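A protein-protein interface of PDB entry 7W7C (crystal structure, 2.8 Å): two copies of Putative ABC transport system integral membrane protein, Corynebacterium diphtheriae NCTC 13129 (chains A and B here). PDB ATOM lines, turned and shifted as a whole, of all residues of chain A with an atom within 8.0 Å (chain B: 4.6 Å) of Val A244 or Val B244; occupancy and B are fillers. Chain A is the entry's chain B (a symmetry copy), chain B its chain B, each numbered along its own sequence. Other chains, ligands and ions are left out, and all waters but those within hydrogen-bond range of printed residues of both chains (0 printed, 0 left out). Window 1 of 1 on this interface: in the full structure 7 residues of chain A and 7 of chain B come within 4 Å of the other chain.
Of the printed residues of chain B, Ala A240 touches Ala B240.
Printed residues of chain B within 4 Å of Thr A243: Val B244 (3.9 Å).
Printed residues of chain B within 4 Å of Gln A248: Leu B247 (3.6 Å).
Printed residues of chain A within 4 Å of Thr B243: Val A244 (3.9 Å).
Of chain A, only Thr A243 and Val A244 come within 4 Å of Val B244.
Of the printed residues of chain A, Leu B247 touches Leu A247 and Gln A248.
The nearest residue of chain B that does not touch Val A244 is Leu B247 (4.1 Å).
The nearest printed residue of chain B that does not touch Ala A240 is Val B244 (5.1 Å).
Of the 9 printed residues of chain B, 5 touch a printed residue of chain A.
Printed residues of chain B that touch a printed residue of chain A: Ala B240, Thr B243, Val B244, Leu B247 and Gln B248.
Hydrophobic or aromatic side chains of chain B within 4 Å of the printed part of chain A: Ala B240, Val B244 and Leu B247.
Of the 16 printed residues of chain A, 5 touch a printed residue of chain B.
Among the printed residues, no Asp or Glu carboxylate lies within 4 Å of a Lys or Arg side-chain nitrogen of the other chain.
The side-chain hydroxyl (OG1) of Thr B243 is in hydrogen-bond range of the backbone carbonyl oxygen (O) of Ala B240, at 2.8 Å.
The backbone carbonyl oxygen of Val A239 is in hydrogen-bond range of the side-chain hydroxyl of Thr A243 (3.1 Å).
OG1 of Thr A243 is in hydrogen-bond range of O of Ala A240 (2.8 Å).
The backbone carbonyl oxygen (O) of Leu A247 is in hydrogen-bond range of the side-chain hydroxyl (OG1) of Thr A250, 2.9 Å away.
Among the printed residues, pairs that only touch across the chains: Ala A240 with Ala B240 (3.5 Å), Thr A243 with Val B244 (3.9 Å), Val A244 with Thr B243 (3.9 Å), Val A244 with Val B244 (3.8 Å), Leu A247 with Leu B247 (3.7 Å), Leu A247 with Gln B248 (3.6 Å) and Gln A248 with Leu B247 (3.6 Å).
Ala A240 touches its own counterpart, Ala B240.
Thr A243 touches Val B244, and with the chains exchanged Val A244 touches Thr B243.
Val A244 touches its own counterpart, Val B244.
Leu B247 touches its own counterpart, Leu A247.
Positions printed for both chains: 240, 241, 242, 243, 244, 245, 246, 247 and 248.
Of the 7 pairs that touch across the chains among the printed residues, 7 have their exchanged pair printed and touching as well.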
ATOM      1  N   ARG A  14      30.103 -20.637  14.638  1.00  0.00           N
ATOM      2  CA  ARG A  14      28.815 -20.431  13.979  1.00  0.00           C
ATOM      3  C   ARG A  14      28.857 -19.223  13.048  1.00  0.00           C
ATOM      4  O   ARG A  14      28.343 -19.271  11.919  1.00  0.00           O
ATOM      5  CB  ARG A  14      27.721 -20.267  15.037  1.00  0.00           C
ATOM      6  CG  ARG A  14      26.298 -20.179  14.507  1.00  0.00           C
ATOM      7  CD  ARG A  14      25.672 -21.557  14.320  1.00  0.00           C
ATOM      8  NE  ARG A  14      24.218 -21.485  14.191  1.00  0.00           N
ATOM      9  CZ  ARG A  14      23.432 -22.534  13.973  1.00  0.00           C
ATOM     10  NH1 ARG A  14      23.959 -23.745  13.854  1.00  0.00           N
ATOM     11  NH2 ARG A  14      22.118 -22.373  13.872  1.00  0.00           N
ATOM     12  N   VAL A 237      18.046 -16.951   4.114  1.00  0.00           N
ATOM     13  CA  VAL A 237      19.058 -17.556   4.981  1.00  0.00           C
ATOM     14  C   VAL A 237      19.435 -16.596   6.103  1.00  0.00           C
ATOM     15  O   VAL A 237      19.540 -16.987   7.279  1.00  0.00           O
ATOM     16  CB  VAL A 237      20.292 -17.975   4.160  1.00  0.00           C
ATOM     17  CG1 VAL A 237      21.464 -18.293   5.078  1.00  0.00           C
ATOM     18  CG2 VAL A 237      19.964 -19.171   3.278  1.00  0.00           C
ATOM     19  N   THR A 238      19.655 -15.324   5.753  1.00  0.00           N
ATOM     20  CA  THR A 238      19.979 -14.327   6.769  1.00  0.00           C
ATOM     21  C   THR A 238      18.858 -14.209   7.795  1.00  0.00           C
ATOM     22  O   THR A 238      19.111 -14.189   9.007  1.00  0.00           O
ATOM     23  CB  THR A 238      20.254 -12.969   6.120  1.00  0.00           C
ATOM     24  OG1 THR A 238      19.128 -12.574   5.329  1.00  0.00           O
ATOM     25  CG2 THR A 238      21.495 -13.035   5.245  1.00  0.00           C
ATOM     26  N   VAL A 239      17.610 -14.130   7.323  1.00  0.00           N
ATOM     27  CA  VAL A 239      16.471 -13.970   8.227  1.00  0.00           C
ATOM     28  C   VAL A 239      16.388 -15.143   9.196  1.00  0.00           C
ATOM     29  O   VAL A 239      16.203 -14.962  10.407  1.00  0.00           O
ATOM     30  CB  VAL A 239      15.165 -13.810   7.425  1.00  0.00           C
ATOM     31  CG1 VAL A 239      13.959 -13.993   8.330  1.00  0.00           C
ATOM     32  CG2 VAL A 239      15.121 -12.447   6.761  1.00  0.00           C
ATOM     33  N   ALA A 240      16.518 -16.364   8.673  1.00  0.00           N
ATOM     34  CA  ALA A 240      16.438 -17.554   9.513  1.00  0.00           C
ATOM     35  C   ALA A 240      17.517 -17.540  10.589  1.00  0.00           C
ATOM     36  O   ALA A 240      17.225 -17.672  11.793  1.00  0.00           O
ATOM     37  CB  ALA A 240      16.562 -18.805   8.643  1.00  0.00           C
ATOM     38  N   PHE A 241      18.780 -17.404  10.166  1.00  0.00           N
ATOM     39  CA  PHE A 241      19.874 -17.442  11.129  1.00  0.00           C
ATOM     40  C   PHE A 241      19.719 -16.357  12.183  1.00  0.00           C
ATOM     41  O   PHE A 241      19.963 -16.599  13.372  1.00  0.00           O
ATOM     42  CB  PHE A 241      21.224 -17.300  10.429  1.00  0.00           C
ATOM     43  CG  PHE A 241      22.361 -17.046  11.382  1.00  0.00           C
ATOM     44  CD1 PHE A 241      22.883 -18.078  12.144  1.00  0.00           C
ATOM     45  CD2 PHE A 241      22.886 -15.772  11.536  1.00  0.00           C
ATOM     46  CE1 PHE A 241      23.916 -17.849  13.032  1.00  0.00           C
ATOM     47  CE2 PHE A 241      23.922 -15.537  12.424  1.00  0.00           C
ATOM     48  CZ  PHE A 241      24.438 -16.578  13.172  1.00  0.00           C
ATOM     49  N   LEU A 242      19.299 -15.157  11.775  1.00  0.00           N
ATOM     50  CA  LEU A 242      19.257 -14.054  12.722  1.00  0.00           C
ATOM     51  C   LEU A 242      18.088 -14.163  13.688  1.00  0.00           C
ATOM     52  O   LEU A 242      18.242 -13.806  14.862  1.00  0.00           O
ATOM     53  CB  LEU A 242      19.233 -12.729  11.966  1.00  0.00           C
ATOM     54  CG  LEU A 242      20.613 -12.421  11.375  1.00  0.00           C
ATOM     55  CD1 LEU A 242      20.531 -11.337  10.321  1.00  0.00           C
ATOM     56  CD2 LEU A 242      21.593 -12.034  12.475  1.00  0.00           C
ATOM     57  N   THR A 243      16.928 -14.670  13.247  1.00  0.00           N
ATOM     58  CA  THR A 243      15.859 -14.914  14.210  1.00  0.00           C
ATOM     59  C   THR A 243      16.286 -15.952  15.236  1.00  0.00           C
ATOM     60  O   THR A 243      16.036 -15.779  16.436  1.00  0.00           O
ATOM     61  CB  THR A 243      14.563 -15.354  13.520  1.00  0.00           C
ATOM     62  OG1 THR A 243      14.801 -16.524  12.731  1.00  0.00           O
ATOM     63  CG2 THR A 243      14.004 -14.242  12.647  1.00  0.00           C
ATOM     64  N   VAL A 244      16.959 -17.023  14.796  1.00  0.00           N
ATOM     65  CA  VAL A 244      17.398 -18.029  15.765  1.00  0.00           C
ATOM     66  C   VAL A 244      18.417 -17.433  16.735  1.00  0.00           C
ATOM     67  O   VAL A 244      18.337 -17.644  17.956  1.00  0.00           O
ATOM     68  CB  VAL A 244      17.949 -19.274  15.047  1.00  0.00           C
ATOM     69  CG1 VAL A 244      18.505 -20.266  16.058  1.00  0.00           C
ATOM     70  CG2 VAL A 244      16.854 -19.922  14.218  1.00  0.00           C
ATOM     71  N   TRP A 245      19.366 -16.653  16.212  1.00  0.00           N
ATOM     72  CA  TRP A 245      20.395 -16.047  17.053  1.00  0.00           C
ATOM     73  C   TRP A 245      19.785 -15.106  18.087  1.00  0.00           C
ATOM     74  O   TRP A 245      20.147 -15.144  19.269  1.00  0.00           O
ATOM     75  CB  TRP A 245      21.405 -15.312  16.172  1.00  0.00           C
ATOM     76  CG  TRP A 245      22.448 -14.549  16.926  1.00  0.00           C
ATOM     77  CD1 TRP A 245      22.611 -13.194  16.955  1.00  0.00           C
ATOM     78  CD2 TRP A 245      23.477 -15.095  17.758  1.00  0.00           C
ATOM     79  NE1 TRP A 245      23.682 -12.862  17.749  1.00  0.00           N
ATOM     80  CE2 TRP A 245      24.228 -14.011  18.259  1.00  0.00           C
ATOM     81  CE3 TRP A 245      23.838 -16.395  18.127  1.00  0.00           C
ATOM     82  CZ2 TRP A 245      25.315 -14.187  19.113  1.00  0.00           C
ATOM     83  CZ3 TRP A 245      24.918 -16.568  18.974  1.00  0.00           C
ATOM     84  CH2 TRP A 245      25.646 -15.468  19.458  1.00  0.00           C
ATOM     85  N   THR A 246      18.844 -14.260  17.662  1.00  0.00           N
ATOM     86  CA  THR A 246      18.200 -13.327  18.582  1.00  0.00           C
ATOM     87  C   THR A 246      17.378 -14.059  19.640  1.00  0.00           C
ATOM     88  O   THR A 246      17.428 -13.710  20.834  1.00  0.00           O
ATOM     89  CB  THR A 246      17.324 -12.359  17.786  1.00  0.00           C
ATOM     90  OG1 THR A 246      18.155 -11.515  16.977  1.00  0.00           O
ATOM     91  CG2 THR A 246      16.480 -11.511  18.711  1.00  0.00           C
ATOM     92  N   LEU A 247      16.607 -15.071  19.223  1.00  0.00           N
ATOM     93  CA  LEU A 247      15.827 -15.860  20.168  1.00  0.00           C
ATOM     94  C   LEU A 247      16.719 -16.550  21.188  1.00  0.00           C
ATOM     95  O   LEU A 247      16.301 -16.775  22.330  1.00  0.00           O
ATOM     96  CB  LEU A 247      14.990 -16.887  19.407  1.00  0.00           C
ATOM     97  CG  LEU A 247      13.994 -17.744  20.186  1.00  0.00           C
ATOM     98  CD1 LEU A 247      13.048 -16.865  20.992  1.00  0.00           C
ATOM     99  CD2 LEU A 247      13.219 -18.629  19.229  1.00  0.00           C
ATOM    100  N   GLN A 248      17.945 -16.903  20.798  1.00  0.00           N
ATOM    101  CA  GLN A 248      18.875 -17.466  21.769  1.00  0.00           C
ATOM    102  C   GLN A 248      19.501 -16.391  22.655  1.00  0.00           C
ATOM    103  O   GLN A 248      19.827 -16.665  23.814  1.00  0.00           O
ATOM    104  CB  GLN A 248      19.952 -18.279  21.048  1.00  0.00           C
ATOM    105  CG  GLN A 248      19.420 -19.581  20.460  1.00  0.00           C
ATOM    106  CD  GLN A 248      20.480 -20.384  19.727  1.00  0.00           C
ATOM    107  OE1 GLN A 248      20.806 -21.505  20.119  1.00  0.00           O
ATOM    108  NE2 GLN A 248      21.015 -19.818  18.650  1.00  0.00           N
ATOM    109  N   ARG A 249      19.661 -15.168  22.138  1.00  0.00           N
ATOM    110  CA  ARG A 249      20.226 -14.064  22.917  1.00  0.00           C
ATOM    111  C   ARG A 249      19.242 -13.452  23.907  1.00  0.00           C
ATOM    112  O   ARG A 249      19.659 -12.615  24.726  1.00  0.00           O
ATOM    113  CB  ARG A 249      20.705 -12.947  21.997  1.00  0.00           C
ATOM    114  CG  ARG A 249      21.870 -13.270  21.116  1.00  0.00           C
ATOM    115  CD  ARG A 249      22.126 -12.061  20.253  1.00  0.00           C
ATOM    116  NE  ARG A 249      22.375 -10.863  21.048  1.00  0.00           N
ATOM    117  CZ  ARG A 249      22.170  -9.626  20.609  1.00  0.00           C
ATOM    118  NH1 ARG A 249      21.695  -9.427  19.386  1.00  0.00           N
ATOM    119  NH2 ARG A 249      22.429  -8.589  21.396  1.00  0.00           N
ATOM    120  N   THR A 250      17.957 -13.809  23.804  1.00  0.00           N
ATOM    121  CA  THR A 250      16.902 -13.199  24.619  1.00  0.00           C
ATOM    122  C   THR A 250      17.298 -12.852  26.057  1.00  0.00           C
ATOM    123  O   THR A 250      17.036 -11.738  26.518  1.00  0.00           O
ATOM    124  CB  THR A 250      15.666 -14.105  24.632  1.00  0.00           C
ATOM    125  OG1 THR A 250      16.055 -15.456  24.914  1.00  0.00           O
ATOM    126  CG2 THR A 250      14.945 -14.045  23.294  1.00  0.00           C
ATOM    127  N   ALA A 327      14.209  -9.507  11.262  1.00  0.00           N
ATOM    128  CA  ALA A 327      14.494 -10.562  12.228  1.00  0.00           C
ATOM    129  C   ALA A 327      14.502 -10.034  13.659  1.00  0.00           C
ATOM    130  O   ALA A 327      13.879 -10.622  14.552  1.00  0.00           O
ATOM    131  CB  ALA A 327      15.830 -11.226  11.893  1.00  0.00           C
ATOM    132  N   ALA B 240      14.043 -23.570   8.703  1.00  0.00           N
ATOM    133  CA  ALA B 240      14.033 -22.342   9.490  1.00  0.00           C
ATOM    134  C   ALA B 240      12.841 -22.308  10.440  1.00  0.00           C
ATOM    135  O   ALA B 240      12.997 -22.120  11.661  1.00  0.00           O
ATOM    136  CB  ALA B 240      14.009 -21.133   8.555  1.00  0.00           C
ATOM    137  N   PHE B 241      11.632 -22.468   9.886  1.00  0.00           N
ATOM    138  CA  PHE B 241      10.438 -22.387  10.719  1.00  0.00           C
ATOM    139  C   PHE B 241      10.472 -23.422  11.833  1.00  0.00           C
ATOM    140  O   PHE B 241      10.099 -23.126  12.975  1.00  0.00           O
ATOM    141  CB  PHE B 241       9.173 -22.565   9.881  1.00  0.00           C
ATOM    142  CG  PHE B 241       7.938 -22.777  10.713  1.00  0.00           C
ATOM    143  CD1 PHE B 241       7.337 -21.713  11.364  1.00  0.00           C
ATOM    144  CD2 PHE B 241       7.395 -24.044  10.867  1.00  0.00           C
ATOM    145  CE1 PHE B 241       6.211 -21.903  12.141  1.00  0.00           C
ATOM    146  CE2 PHE B 241       6.266 -24.241  11.644  1.00  0.00           C
ATOM    147  CZ  PHE B 241       5.673 -23.168  12.281  1.00  0.00           C
ATOM    148  N   LEU B 242      10.932 -24.639  11.530  1.00  0.00           N
ATOM    149  CA  LEU B 242      10.866 -25.696  12.526  1.00  0.00           C
ATOM    150  C   LEU B 242      11.921 -25.540  13.610  1.00  0.00           C
ATOM    151  O   LEU B 242      11.637 -25.842  14.774  1.00  0.00           O
ATOM    152  CB  LEU B 242      10.970 -27.055  11.840  1.00  0.00           C
ATOM    153  CG  LEU B 242       9.664 -27.394  11.114  1.00  0.00           C
ATOM    154  CD1 LEU B 242       9.859 -28.525  10.127  1.00  0.00           C
ATOM    155  CD2 LEU B 242       8.566 -27.732  12.115  1.00  0.00           C
ATOM    156  N   THR B 243      13.124 -25.051  13.276  1.00  0.00           N
ATOM    157  CA  THR B 243      14.081 -24.760  14.340  1.00  0.00           C
ATOM    158  C   THR B 243      13.545 -23.676  15.264  1.00  0.00           C
ATOM    159  O   THR B 243      13.660 -23.793  16.490  1.00  0.00           O
ATOM    160  CB  THR B 243      15.446 -24.349  13.778  1.00  0.00           C
ATOM    161  OG1 THR B 243      15.300 -23.217  12.914  1.00  0.00           O
ATOM    162  CG2 THR B 243      16.095 -25.499  13.025  1.00  0.00           C
ATOM    163  N   VAL B 244      12.928 -22.629  14.702  1.00  0.00           N
ATOM    164  CA  VAL B 244      12.386 -21.580  15.569  1.00  0.00           C
ATOM    165  C   VAL B 244      11.265 -22.133  16.446  1.00  0.00           C
ATOM    166  O   VAL B 244      11.209 -21.865  17.657  1.00  0.00           O
ATOM    167  CB  VAL B 244      11.921 -20.371  14.737  1.00  0.00           C
ATOM    168  CG1 VAL B 244      11.259 -19.335  15.633  1.00  0.00           C
ATOM    169  CG2 VAL B 244      13.103 -19.759  14.006  1.00  0.00           C
ATOM    170  N   TRP B 245      10.377 -22.939  15.859  1.00  0.00           N
ATOM    171  CA  TRP B 245       9.260 -23.507  16.607  1.00  0.00           C
ATOM    172  C   TRP B 245       9.749 -24.399  17.745  1.00  0.00           C
ATOM    173  O   TRP B 245       9.258 -24.307  18.877  1.00  0.00           O
ATOM    174  CB  TRP B 245       8.352 -24.286  15.654  1.00  0.00           C
ATOM    175  CG  TRP B 245       7.230 -25.015  16.323  1.00  0.00           C
ATOM    176  CD1 TRP B 245       7.062 -26.368  16.396  1.00  0.00           C
ATOM    177  CD2 TRP B 245       6.116 -24.434  17.010  1.00  0.00           C
ATOM    178  NE1 TRP B 245       5.908 -26.665  17.081  1.00  0.00           N
ATOM    179  CE2 TRP B 245       5.312 -25.496  17.474  1.00  0.00           C
ATOM    180  CE3 TRP B 245       5.720 -23.119  17.276  1.00  0.00           C
ATOM    181  CZ2 TRP B 245       4.137 -25.283  18.193  1.00  0.00           C
ATOM    182  CZ3 TRP B 245       4.553 -22.910  17.988  1.00  0.00           C
ATOM    183  CH2 TRP B 245       3.774 -23.988  18.439  1.00  0.00           C
ATOM    184  N   THR B 246      10.729 -25.261  17.466  1.00  0.00           N
ATOM    185  CA  THR B 246      11.264 -26.148  18.494  1.00  0.00           C
ATOM    186  C   THR B 246      11.967 -25.366  19.602  1.00  0.00           C
ATOM    187  O   THR B 246      11.783 -25.659  20.798  1.00  0.00           O
ATOM    188  CB  THR B 246      12.221 -27.150  17.846  1.00  0.00           C
ATOM    189  OG1 THR B 246      11.483 -28.032  16.990  1.00  0.00           O
ATOM    190  CG2 THR B 246      12.955 -27.952  18.898  1.00  0.00           C
ATOM    191  N   LEU B 247      12.782 -24.373  19.226  1.00  0.00           N
ATOM    192  CA  LEU B 247      13.453 -23.539  20.214  1.00  0.00           C
ATOM    193  C   LEU B 247      12.456 -22.805  21.096  1.00  0.00           C
ATOM    194  O   LEU B 247      12.746 -22.526  22.266  1.00  0.00           O
ATOM    195  CB  LEU B 247      14.373 -22.546  19.504  1.00  0.00           C
ATOM    196  CG  LEU B 247      15.278 -21.652  20.348  1.00  0.00           C
ATOM    197  CD1 LEU B 247      16.127 -22.490  21.294  1.00  0.00           C
ATOM    198  CD2 LEU B 247      16.157 -20.809  19.444  1.00  0.00           C
ATOM    199  N   GLN B 248      11.282 -22.473  20.556  1.00  0.00           N
ATOM    200  CA  GLN B 248      10.251 -21.868  21.392  1.00  0.00           C
ATOM    201  C   GLN B 248       9.528 -22.903  22.251  1.00  0.00           C
ATOM    202  O   GLN B 248       9.077 -22.576  23.353  1.00  0.00           O
ATOM    203  CB  GLN B 248       9.263 -21.093  20.518  1.00  0.00           C
ATOM    204  CG  GLN B 248       9.860 -19.817  19.934  1.00  0.00           C
ATOM    205  CD  GLN B 248       8.890 -19.052  19.052  1.00  0.00           C
ATOM    206  OE1 GLN B 248       8.526 -17.915  19.352  1.00  0.00           O
ATOM    207  NE2 GLN B 248       8.477 -19.668  17.949  1.00  0.00           N
